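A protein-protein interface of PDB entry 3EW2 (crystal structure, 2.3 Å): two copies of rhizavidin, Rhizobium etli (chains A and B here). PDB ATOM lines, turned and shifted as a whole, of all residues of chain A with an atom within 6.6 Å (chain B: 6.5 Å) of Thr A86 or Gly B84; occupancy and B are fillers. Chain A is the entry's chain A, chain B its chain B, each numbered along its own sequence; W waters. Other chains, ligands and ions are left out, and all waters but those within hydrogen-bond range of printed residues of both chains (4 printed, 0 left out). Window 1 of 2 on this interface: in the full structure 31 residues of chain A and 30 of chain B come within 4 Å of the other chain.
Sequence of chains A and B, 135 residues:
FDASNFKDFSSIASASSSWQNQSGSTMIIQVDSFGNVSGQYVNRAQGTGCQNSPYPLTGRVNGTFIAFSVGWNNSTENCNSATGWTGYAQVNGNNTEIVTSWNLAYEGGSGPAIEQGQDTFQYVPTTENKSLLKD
Printed residues of chain B that touch a printed residue of chain A: Phe B68, Ser B69, Ala B82, Thr B83, Gly B84, Thr B86, Ser B101, Trp B102, Asn B103, Ala B105 and Ile B114. Hydrophobic or aromatic side chains of chain B that line the printed part of chain A: Ala B82, Ala B105 and Ile B114. Of the 15 printed residues of chain A, 11 touch a printed residue of chain B. Hydrophobic or aromatic side chains of chain A within 4 Å of the printed part of chain B: Ala A67 and Tyr A88.
Gly A84 touches Thr B86, and with the chains exchanged Thr A86 touches Gly B84. Thr A86 touches Asn B103, and with the chains exchanged Asn A103 touches Thr B86. Ser A101 touches Asn B103, and with the chains exchanged Asn A103 touches Ser B101. Asn A103 touches Trp B102, but with the chains exchanged Trp A102 does not touch Asn B103 (4.1 Å). Positions printed for both chains: 68, 69, 84, 85, 86, 101, 102 and 103. Of the 23 pairs that touch across the chains among the printed residues, 10 have their exchanged pair printed and touching as well.
O of Asn A103 lies within hydrogen-bond range of OG1 of Thr B86. OG of Ser B69 sits at hydrogen-bond distance from OG of Ser A69, at 2.6 Å. N of Gly B84 lies within hydrogen-bond range of OG1 of Thr A86 (3.1 Å). The side-chain hydroxyl of Thr B86 lies within hydrogen-bond range of the backbone NH of Gly A84 (3.1 Å). ND2 of Asn A103 lies close to ND2 of Asn B103, at 3.1 Å. O of Ala A67 lies within hydrogen-bond range of OG of Ser B69. The side-chain hydroxyl (OG1) of Thr A86 is in hydrogen-bond range of the backbone carbonyl oxygen (O) of Asn B103 (3.5 Å).
Among the printed residues, merely in contact across the chains: Ile A66 with Ala B82 (3.7 Å), Ala A67 with Thr B83 (3.5 Å), Ala A67 with Gly B84 (3.8 Å), Phe A68 with Ser B69 (3.5 Å), Ser A69 with Phe B68 (3.4 Å), Thr A86 with Ala B82 (3.3 Å), Thr A86 with Thr B83 (3.98 Å), Thr A86 with Ala B105 (3.6 Å), Thr A86 with Ile B114 (3.8 Å), Gly A87 with Ala B105 (3.7 Å), Tyr A88 with Ile B114 (3.8 Å), Val A99 with Ile B114 (3.96 Å), Ser A101 with Asn B103 (3.7 Å), Ser A101 with Ile B114 (3.5 Å), Asn A103 with Ser B101 (3.6 Å) and Asn A103 with Trp B102 (3.9 Å).
The backbone carbonyl oxygen (O) of Ala B82 sits at hydrogen-bond distance from the backbone NH (N) of Ala B105, at 2.9 Å. N of Gly A87 sits at hydrogen-bond distance from O of Ile A66 (2.9 Å). N of Val A99 lies within hydrogen-bond range of O of Tyr A88 (3.1 Å). The side-chain hydroxyl of Thr B83 lies within hydrogen-bond range of the indole nitrogen of Trp B72, at 2.7 Å. The backbone carbonyl oxygen (O) of Gly A84 lies within hydrogen-bond range of the backbone NH (N) of Asn A103. The backbone NH (N) of Thr A86 lies within hydrogen-bond range of the backbone carbonyl oxygen (O) of Ser A101, at 2.9 Å.
Water W3 lies within hydrogen-bond range of the side-chain hydroxyl of Thr A86 (2.5 Å), the backbone carbonyl oxygen of Gly A84 (3.2 Å) and the side-chain amide nitrogen of Asn B103 (3.3 Å). Water W2 lies within hydrogen-bond range of the side-chain hydroxyl of Thr B86 (2.7 Å), the side-chain amide nitrogen of Asn A103 (2.9 Å) and the backbone carbonyl oxygen of Gly B84 (3.4 Å). Water W1 lies within hydrogen-bond range of O of Trp A102, OD1 of Asn A103 and ND2 of Asn B103. Water W4 lies within hydrogen-bond range of the backbone carbonyl oxygen (O) of Trp B102 (3.3 Å) and the side-chain amide nitrogen (ND2) of Asn A103 (3.4 Å).
Printed residues of chain B within 4 Å of Ile A66: Ala B82 (3.7 Å). Of the printed residues of chain B, Ser A69 touches Phe B68 (3.4 Å) and Ser B69 (2.6 Å). Printed residues of chain B within 4 Å of Thr A86: Ala B82, Thr B83, Gly B84, Asn B103, Ala B105 and Ile B114. Of chain A, only Ala A67 (3.8 Å) and Thr A86 (3.1 Å) come within 4 Å of Gly B84. Printed residues of chain A within 4 Å of Ile B114: Thr A86, Tyr A88, Val A99 and Ser A101. The nearest printed residue of chain B that does not touch Thr A86 is Leu B104 (4.5 Å). The nearest residue of chain A that does not touch Gly B84 is Trp A85 (4.9 Å). The nearest printed residue of chain B that does not touch Tyr A88 is Ala B105 (4.8 Å).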
ATOM      1  N   ILE A  66     -27.608 -12.413   4.157  1.00  0.00           N
ATOM      2  CA  ILE A  66     -28.218 -11.777   3.004  1.00  0.00           C
ATOM      3  C   ILE A  66     -27.453 -10.527   2.653  1.00  0.00           C
ATOM      4  O   ILE A  66     -26.928  -9.867   3.539  1.00  0.00           O
ATOM      5  CB  ILE A  66     -29.702 -11.360   3.323  1.00  0.00           C
ATOM      6  CG1 ILE A  66     -30.466 -10.823   2.091  1.00  0.00           C
ATOM      7  CG2 ILE A  66     -29.773 -10.373   4.513  1.00  0.00           C
ATOM      8  CD1 ILE A  66     -32.050 -10.815   2.318  1.00  0.00           C
ATOM      9  N   ALA A  67     -27.403 -10.222   1.363  1.00  0.00           N
ATOM     10  CA  ALA A  67     -26.931  -8.957   0.888  1.00  0.00           C
ATOM     11  C   ALA A  67     -27.896  -8.475  -0.207  1.00  0.00           C
ATOM     12  O   ALA A  67     -28.368  -9.279  -1.066  1.00  0.00           O
ATOM     13  CB  ALA A  67     -25.482  -9.112   0.294  1.00  0.00           C
ATOM     14  N   PHE A  68     -28.205  -7.186  -0.202  1.00  0.00           N
ATOM     15  CA  PHE A  68     -29.037  -6.641  -1.278  1.00  0.00           C
ATOM     16  C   PHE A  68     -28.576  -5.258  -1.729  1.00  0.00           C
ATOM     17  O   PHE A  68     -27.832  -4.612  -1.010  1.00  0.00           O
ATOM     18  CB  PHE A  68     -30.574  -6.706  -0.940  1.00  0.00           C
ATOM     19  CG  PHE A  68     -30.975  -5.996   0.359  1.00  0.00           C
ATOM     20  CD1 PHE A  68     -30.862  -6.656   1.598  1.00  0.00           C
ATOM     21  CD2 PHE A  68     -31.450  -4.678   0.346  1.00  0.00           C
ATOM     22  CE1 PHE A  68     -31.245  -6.028   2.782  1.00  0.00           C
ATOM     23  CE2 PHE A  68     -31.827  -4.042   1.528  1.00  0.00           C
ATOM     24  CZ  PHE A  68     -31.740  -4.734   2.745  1.00  0.00           C
ATOM     25  N   SER A  69     -29.009  -4.834  -2.925  1.00  0.00           N
ATOM     26  CA  SER A  69     -28.446  -3.695  -3.640  1.00  0.00           C
ATOM     27  C   SER A  69     -29.614  -2.861  -4.185  1.00  0.00           C
ATOM     28  O   SER A  69     -30.627  -3.428  -4.590  1.00  0.00           O
ATOM     29  CB  SER A  69     -27.568  -4.176  -4.832  1.00  0.00           C
ATOM     30  OG  SER A  69     -26.845  -5.387  -4.549  1.00  0.00           O
ATOM     31  N   GLY A  84     -25.675  -0.696  -0.924  1.00  0.00           N
ATOM     32  CA  GLY A  84     -25.722  -2.100  -0.673  1.00  0.00           C
ATOM     33  C   GLY A  84     -25.751  -2.366   0.823  1.00  0.00           C
ATOM     34  O   GLY A  84     -25.076  -1.656   1.613  1.00  0.00           O
ATOM     35  N   TRP A  85     -26.503  -3.390   1.203  1.00  0.00           N
ATOM     36  CA  TRP A  85     -26.732  -3.747   2.589  1.00  0.00           C
ATOM     37  C   TRP A  85     -26.245  -5.171   2.733  1.00  0.00           C
ATOM     38  O   TRP A  85     -26.469  -5.968   1.835  1.00  0.00           O
ATOM     39  CB  TRP A  85     -28.262  -3.805   2.920  1.00  0.00           C
ATOM     40  CG  TRP A  85     -28.988  -2.513   3.114  1.00  0.00           C
ATOM     41  CD1 TRP A  85     -29.276  -1.934   4.294  1.00  0.00           C
ATOM     42  CD2 TRP A  85     -29.519  -1.635   2.094  1.00  0.00           C
ATOM     43  NE1 TRP A  85     -29.957  -0.757   4.104  1.00  0.00           N
ATOM     44  CE2 TRP A  85     -30.133  -0.553   2.764  1.00  0.00           C
ATOM     45  CE3 TRP A  85     -29.548  -1.675   0.687  1.00  0.00           C
ATOM     46  CZ2 TRP A  85     -30.762   0.493   2.094  1.00  0.00           C
ATOM     47  CZ3 TRP A  85     -30.177  -0.645   0.006  1.00  0.00           C
ATOM     48  CH2 TRP A  85     -30.794   0.427   0.720  1.00  0.00           C
ATOM     49  N   THR A  86     -25.711  -5.522   3.891  1.00  0.00           N
ATOM     50  CA  THR A  86     -25.310  -6.896   4.171  1.00  0.00           C
ATOM     51  C   THR A  86     -25.584  -7.193   5.604  1.00  0.00           C
ATOM     52  O   THR A  86     -25.143  -6.440   6.487  1.00  0.00           O
ATOM     53  CB  THR A  86     -23.740  -7.110   3.952  1.00  0.00           C
ATOM     54  OG1 THR A  86     -23.337  -6.459   2.750  1.00  0.00           O
ATOM     55  CG2 THR A  86     -23.396  -8.591   3.851  1.00  0.00           C
ATOM     56  N   GLY A  87     -26.277  -8.291   5.871  1.00  0.00           N
ATOM     57  CA  GLY A  87     -26.436  -8.678   7.239  1.00  0.00           C
ATOM     58  C   GLY A  87     -26.941 -10.073   7.443  1.00  0.00           C
ATOM     59  O   GLY A  87     -26.731 -10.974   6.625  1.00  0.00           O
ATOM     60  N   TYR A  88     -27.589 -10.263   8.574  1.00  0.00           N
ATOM     61  CA  TYR A  88     -28.128 -11.564   8.926  1.00  0.00           C
ATOM     62  C   TYR A  88     -29.492 -11.372   9.576  1.00  0.00           C
ATOM     63  O   TYR A  88     -29.721 -10.364  10.236  1.00  0.00           O
ATOM     64  CB  TYR A  88     -27.174 -12.241   9.882  1.00  0.00           C
ATOM     65  CG  TYR A  88     -26.775 -11.382  11.061  1.00  0.00           C
ATOM     66  CD1 TYR A  88     -25.725 -10.469  10.971  1.00  0.00           C
ATOM     67  CD2 TYR A  88     -27.448 -11.495  12.287  1.00  0.00           C
ATOM     68  CE1 TYR A  88     -25.352  -9.701  12.063  1.00  0.00           C
ATOM     69  CE2 TYR A  88     -27.090 -10.700  13.399  1.00  0.00           C
ATOM     70  CZ  TYR A  88     -26.038  -9.831  13.279  1.00  0.00           C
ATOM     71  OH  TYR A  88     -25.700  -9.047  14.355  1.00  0.00           O
ATOM     72  N   ILE A  98     -33.605  -8.069  10.623  1.00  0.00           N
ATOM     73  CA  ILE A  98     -32.377  -8.083   9.843  1.00  0.00           C
ATOM     74  C   ILE A  98     -31.403  -6.987  10.282  1.00  0.00           C
ATOM     75  O   ILE A  98     -31.679  -5.823  10.109  1.00  0.00           O
ATOM     76  CB  ILE A  98     -32.652  -8.032   8.318  1.00  0.00           C
ATOM     77  CG1 ILE A  98     -33.869  -8.932   7.995  1.00  0.00           C
ATOM     78  CG2 ILE A  98     -31.314  -8.294   7.557  1.00  0.00           C
ATOM     79  CD1 ILE A  98     -34.009  -9.426   6.627  1.00  0.00           C
ATOM     80  N   VAL A  99     -30.271  -7.401  10.848  1.00  0.00           N
ATOM     81  CA  VAL A  99     -29.183  -6.491  11.270  1.00  0.00           C
ATOM     82  C   VAL A  99     -28.267  -6.269  10.063  1.00  0.00           C
ATOM     83  O   VAL A  99     -27.698  -7.220   9.546  1.00  0.00           O
ATOM     84  CB  VAL A  99     -28.351  -7.129  12.450  1.00  0.00           C
ATOM     85  CG1 VAL A  99     -27.086  -6.292  12.808  1.00  0.00           C
ATOM     86  CG2 VAL A  99     -29.242  -7.440  13.706  1.00  0.00           C
ATOM     87  N   THR A 100     -28.115  -5.031   9.612  1.00  0.00           N
ATOM     88  CA  THR A 100     -27.300  -4.756   8.433  1.00  0.00           C
ATOM     89  C   THR A 100     -26.179  -3.691   8.626  1.00  0.00           C
ATOM     90  O   THR A 100     -26.250  -2.839   9.511  1.00  0.00           O
ATOM     91  CB  THR A 100     -28.174  -4.287   7.215  1.00  0.00           C
ATOM     92  OG1 THR A 100     -28.641  -2.947   7.407  1.00  0.00           O
ATOM     93  CG2 THR A 100     -29.339  -5.213   6.929  1.00  0.00           C
ATOM     94  N   SER A 101     -25.154  -3.738   7.770  1.00  0.00           N
ATOM     95  CA  SER A 101     -24.318  -2.545   7.549  1.00  0.00           C
ATOM     96  C   SER A 101     -24.542  -2.195   6.095  1.00  0.00           C
ATOM     97  O   SER A 101     -24.920  -3.059   5.308  1.00  0.00           O
ATOM     98  CB  SER A 101     -22.817  -2.787   7.830  1.00  0.00           C
ATOM     99  OG  SER A 101     -22.629  -3.483   9.054  1.00  0.00           O
ATOM    100  N   TRP A 102     -24.353  -0.934   5.761  1.00  0.00           N
ATOM    101  CA  TRP A 102     -24.607  -0.476   4.432  1.00  0.00           C
ATOM    102  C   TRP A 102     -23.583   0.539   4.003  1.00  0.00           C
ATOM    103  O   TRP A 102     -22.951   1.172   4.819  1.00  0.00           O
ATOM    104  CB  TRP A 102     -26.062   0.047   4.221  1.00  0.00           C
ATOM    105  CG  TRP A 102     -26.541   1.120   5.168  1.00  0.00           C
ATOM    106  CD1 TRP A 102     -27.361   0.959   6.262  1.00  0.00           C
ATOM    107  CD2 TRP A 102     -26.239   2.517   5.095  1.00  0.00           C
ATOM    108  NE1 TRP A 102     -27.585   2.169   6.865  1.00  0.00           N
ATOM    109  CE2 TRP A 102     -26.911   3.144   6.165  1.00  0.00           C
ATOM    110  CE3 TRP A 102     -25.475   3.304   4.214  1.00  0.00           C
ATOM    111  CZ2 TRP A 102     -26.823   4.524   6.392  1.00  0.00           C
ATOM    112  CZ3 TRP A 102     -25.394   4.659   4.423  1.00  0.00           C
ATOM    113  CH2 TRP A 102     -26.057   5.265   5.520  1.00  0.00           C
ATOM    114  N   ASN A 103     -23.406   0.646   2.696  1.00  0.00           N
ATOM    115  CA  ASN A 103     -22.617   1.673   2.115  1.00  0.00           C
ATOM    116  C   ASN A 103     -23.475   2.334   1.103  1.00  0.00           C
ATOM    117  O   ASN A 103     -24.265   1.689   0.453  1.00  0.00           O
ATOM    118  CB  ASN A 103     -21.359   1.080   1.448  1.00  0.00           C
ATOM    119  CG  ASN A 103     -20.362   0.600   2.470  1.00  0.00           C
ATOM    120  OD1 ASN A 103     -19.868   1.397   3.259  1.00  0.00           O
ATOM    121  ND2 ASN A 103     -20.157  -0.718   2.544  1.00  0.00           N
ATOM    122  N   PHE B  68     -23.526  -4.619  -5.714  1.00  0.00           N
ATOM    123  CA  PHE B  68     -23.835  -5.984  -6.074  1.00  0.00           C
ATOM    124  C   PHE B  68     -23.602  -6.884  -4.868  1.00  0.00           C
ATOM    125  O   PHE B  68     -23.037  -6.462  -3.836  1.00  0.00           O
ATOM    126  CB  PHE B  68     -23.044  -6.417  -7.314  1.00  0.00           C
ATOM    127  CG  PHE B  68     -21.523  -6.282  -7.154  1.00  0.00           C
ATOM    128  CD1 PHE B  68     -20.877  -5.086  -7.451  1.00  0.00           C
ATOM    129  CD2 PHE B  68     -20.765  -7.349  -6.693  1.00  0.00           C
ATOM    130  CE1 PHE B  68     -19.499  -4.957  -7.281  1.00  0.00           C
ATOM    131  CE2 PHE B  68     -19.381  -7.225  -6.526  1.00  0.00           C
ATOM    132  CZ  PHE B  68     -18.757  -6.042  -6.828  1.00  0.00           C
ATOM    133  N   SER B  69     -24.041  -8.119  -4.986  1.00  0.00           N
ATOM    134  CA  SER B  69     -24.305  -8.909  -3.820  1.00  0.00           C
ATOM    135  C   SER B  69     -23.896 -10.306  -4.172  1.00  0.00           C
ATOM    136  O   SER B  69     -24.129 -10.728  -5.294  1.00  0.00           O
ATOM    137  CB  SER B  69     -25.837  -8.915  -3.519  1.00  0.00           C
ATOM    138  OG  SER B  69     -26.318  -7.603  -3.257  1.00  0.00           O
ATOM    139  N   VAL B  70     -23.357 -11.045  -3.209  1.00  0.00           N
ATOM    140  CA  VAL B  70     -23.042 -12.445  -3.450  1.00  0.00           C
ATOM    141  C   VAL B  70     -23.409 -13.211  -2.175  1.00  0.00           C
ATOM    142  O   VAL B  70     -23.052 -12.789  -1.099  1.00  0.00           O
ATOM    143  CB  VAL B  70     -21.451 -12.619  -3.718  1.00  0.00           C
ATOM    144  CG1 VAL B  70     -20.993 -14.031  -3.457  1.00  0.00           C
ATOM    145  CG2 VAL B  70     -21.039 -12.159  -5.123  1.00  0.00           C
ATOM    146  N   TRP B  72     -22.560 -16.754  -0.188  1.00  0.00           N
ATOM    147  CA  TRP B  72     -21.409 -17.649  -0.301  1.00  0.00           C
ATOM    148  C   TRP B  72     -21.811 -19.118  -0.221  1.00  0.00           C
ATOM    149  O   TRP B  72     -21.303 -19.888   0.615  1.00  0.00           O
ATOM    150  CB  TRP B  72     -20.257 -17.255   0.652  1.00  0.00           C
ATOM    151  CG  TRP B  72     -19.707 -15.864   0.359  1.00  0.00           C
ATOM    152  CD1 TRP B  72     -19.881 -14.739   1.116  1.00  0.00           C
ATOM    153  CD2 TRP B  72     -18.917 -15.451  -0.797  1.00  0.00           C
ATOM    154  NE1 TRP B  72     -19.253 -13.657   0.516  1.00  0.00           N
ATOM    155  CE2 TRP B  72     -18.651 -14.068  -0.647  1.00  0.00           C
ATOM    156  CE3 TRP B  72     -18.386 -16.133  -1.915  1.00  0.00           C
ATOM    157  CZ2 TRP B  72     -17.909 -13.327  -1.595  1.00  0.00           C
ATOM    158  CZ3 TRP B  72     -17.640 -15.427  -2.835  1.00  0.00           C
ATOM    159  CH2 TRP B  72     -17.419 -14.013  -2.680  1.00  0.00           C
ATOM    160  N   ALA B  82     -22.541 -13.879   3.441  1.00  0.00           N
ATOM    161  CA  ALA B  82     -22.906 -13.122   2.261  1.00  0.00           C
ATOM    162  C   ALA B  82     -22.079 -11.856   2.263  1.00  0.00           C
ATOM    163  O   ALA B  82     -21.669 -11.399   3.326  1.00  0.00           O
ATOM    164  CB  ALA B  82     -24.410 -12.780   2.319  1.00  0.00           C
ATOM    165  N   THR B  83     -21.844 -11.283   1.082  1.00  0.00           N
ATOM    166  CA  THR B  83     -21.095 -10.056   0.947  1.00  0.00           C
ATOM    167  C   THR B  83     -21.820  -9.094   0.007  1.00  0.00           C
ATOM    168  O   THR B  83     -22.269  -9.502  -1.051  1.00  0.00           O
ATOM    169  CB  THR B  83     -19.630 -10.339   0.375  1.00  0.00           C
ATOM    170  OG1 THR B  83     -18.847 -11.123   1.296  1.00  0.00           O
ATOM    171  CG2 THR B  83     -18.898  -9.053   0.117  1.00  0.00           C
ATOM    172  N   GLY B  84     -21.905  -7.810   0.365  1.00  0.00           N
ATOM    173  CA  GLY B  84     -22.311  -6.784  -0.584  1.00  0.00           C
ATOM    174  C   GLY B  84     -21.250  -5.710  -0.757  1.00  0.00           C
ATOM    175  O   GLY B  84     -20.508  -5.393   0.176  1.00  0.00           O
ATOM    176  N   TRP B  85     -21.194  -5.136  -1.952  1.00  0.00           N
ATOM    177  CA  TRP B  85     -20.218  -4.167  -2.336  1.00  0.00           C
ATOM    178  C   TRP B  85     -20.966  -2.984  -2.886  1.00  0.00           C
ATOM    179  O   TRP B  85     -21.994  -3.163  -3.479  1.00  0.00           O
ATOM    180  CB  TRP B  85     -19.411  -4.693  -3.526  1.00  0.00           C
ATOM    181  CG  TRP B  85     -18.318  -5.708  -3.281  1.00  0.00           C
ATOM    182  CD1 TRP B  85     -16.959  -5.452  -3.138  1.00  0.00           C
ATOM    183  CD2 TRP B  85     -18.461  -7.147  -3.238  1.00  0.00           C
ATOM    184  NE1 TRP B  85     -16.277  -6.646  -2.984  1.00  0.00           N
ATOM    185  CE2 TRP B  85     -17.163  -7.695  -3.044  1.00  0.00           C
ATOM    186  CE3 TRP B  85     -19.547  -8.019  -3.375  1.00  0.00           C
ATOM    187  CZ2 TRP B  85     -16.940  -9.063  -2.978  1.00  0.00           C
ATOM    188  CZ3 TRP B  85     -19.328  -9.368  -3.291  1.00  0.00           C
ATOM    189  CH2 TRP B  85     -18.032  -9.891  -3.106  1.00  0.00           C
ATOM    190  N   THR B  86     -20.418  -1.771  -2.729  1.00  0.00           N
ATOM    191  CA  THR B  86     -21.028  -0.552  -3.270  1.00  0.00           C
ATOM    192  C   THR B  86     -19.856   0.321  -3.675  1.00  0.00           C
ATOM    193  O   THR B  86     -18.896   0.453  -2.916  1.00  0.00           O
ATOM    194  CB  THR B  86     -21.833   0.227  -2.182  1.00  0.00           C
ATOM    195  OG1 THR B  86     -22.592  -0.686  -1.406  1.00  0.00           O
ATOM    196  CG2 THR B  86     -22.730   1.250  -2.791  1.00  0.00           C
ATOM    197  N   SER B 101     -16.544  -0.020  -1.203  1.00  0.00           N
ATOM    198  CA  SER B 101     -16.460  -0.527   0.161  1.00  0.00           C
ATOM    199  C   SER B 101     -17.386  -1.682   0.124  1.00  0.00           C
ATOM    200  O   SER B 101     -18.281  -1.672  -0.714  1.00  0.00           O
ATOM    201  CB  SER B 101     -16.952   0.489   1.202  1.00  0.00           C
ATOM    202  OG  SER B 101     -16.216   1.682   1.089  1.00  0.00           O
ATOM    203  N   TRP B 102     -17.167  -2.658   1.016  1.00  0.00           N
ATOM    204  CA  TRP B 102     -17.898  -3.915   1.090  1.00  0.00           C
ATOM    205  C   TRP B 102     -18.129  -4.350   2.537  1.00  0.00           C
ATOM    206  O   TRP B 102     -17.397  -3.935   3.430  1.00  0.00           O
ATOM    207  CB  TRP B 102     -17.178  -5.061   0.349  1.00  0.00           C
ATOM    208  CG  TRP B 102     -15.711  -5.378   0.701  1.00  0.00           C
ATOM    209  CD1 TRP B 102     -14.587  -5.019  -0.043  1.00  0.00           C
ATOM    210  CD2 TRP B 102     -15.214  -6.167   1.822  1.00  0.00           C
ATOM    211  NE1 TRP B 102     -13.436  -5.525   0.578  1.00  0.00           N
ATOM    212  CE2 TRP B 102     -13.799  -6.232   1.706  1.00  0.00           C
ATOM    213  CE3 TRP B 102     -15.828  -6.822   2.898  1.00  0.00           C
ATOM    214  CZ2 TRP B 102     -12.995  -6.922   2.642  1.00  0.00           C
ATOM    215  CZ3 TRP B 102     -15.036  -7.492   3.835  1.00  0.00           C
ATOM    216  CH2 TRP B 102     -13.625  -7.542   3.698  1.00  0.00           C
ATOM    217  N   ASN B 103     -19.144  -5.171   2.769  1.00  0.00           N
ATOM    218  CA  ASN B 103     -19.325  -5.774   4.083  1.00  0.00           C
ATOM    219  C   ASN B 103     -19.461  -7.226   3.925  1.00  0.00           C
ATOM    220  O   ASN B 103     -20.062  -7.663   2.971  1.00  0.00           O
ATOM    221  CB  ASN B 103     -20.555  -5.231   4.808  1.00  0.00           C
ATOM    222  CG  ASN B 103     -20.317  -3.879   5.335  1.00  0.00           C
ATOM    223  OD1 ASN B 103     -19.522  -3.722   6.262  1.00  0.00           O
ATOM    224  ND2 ASN B 103     -20.907  -2.847   4.675  1.00  0.00           N
ATOM    225  N   LEU B 104     -18.912  -7.975   4.869  1.00  0.00           N
ATOM    226  CA  LEU B 104     -19.026  -9.400   4.839  1.00  0.00           C
ATOM    227  C   LEU B 104     -19.705  -9.851   6.098  1.00  0.00           C
ATOM    228  O   LEU B 104     -19.221  -9.600   7.197  1.00  0.00           O
ATOM    229  CB  LEU B 104     -17.653 -10.025   4.706  1.00  0.00           C
ATOM    230  CG  LEU B 104     -17.406 -11.517   4.940  1.00  0.00           C
ATOM    231  CD1 LEU B 104     -18.270 -12.405   4.043  1.00  0.00           C
ATOM    232  CD2 LEU B 104     -15.918 -11.703   4.640  1.00  0.00           C
ATOM    233  N   ALA B 105     -20.864 -10.493   5.926  1.00  0.00           N
ATOM    234  CA  ALA B 105     -21.653 -10.917   7.058  1.00  0.00           C
ATOM    235  C   ALA B 105     -21.492 -12.419   7.172  1.00  0.00           C
ATOM    236  O   ALA B 105     -21.729 -13.152   6.220  1.00  0.00           O
ATOM    237  CB  ALA B 105     -23.117 -10.518   6.873  1.00  0.00           C
ATOM    238  N   ILE B 114     -20.120  -8.879  11.261  1.00  0.00           N
ATOM    239  CA  ILE B 114     -20.100  -8.226   9.971  1.00  0.00           C
ATOM    240  C   ILE B 114     -18.769  -7.520   9.892  1.00  0.00           C
ATOM    241  O   ILE B 114     -18.538  -6.612  10.653  1.00  0.00           O
ATOM    242  CB  ILE B 114     -21.238  -7.198   9.788  1.00  0.00           C
ATOM    243  CG1 ILE B 114     -22.606  -7.836  10.100  1.00  0.00           C
ATOM    244  CG2 ILE B 114     -21.229  -6.666   8.354  1.00  0.00           C
ATOM    245  CD1 ILE B 114     -23.774  -6.930   9.960  1.00  0.00           C
HETATM  246  O   HOH W   1     -20.373   0.230   6.239  1.00  0.00           O
HETATM  247  O   HOH W   2     -21.590  -2.237   0.557  1.00  0.00           O
HETATM  248  O   HOH W   3     -23.032  -4.051   2.401  1.00  0.00           O
HETATM  249  O   HOH W   4     -17.329  -0.810   4.338  1.00  0.00           O
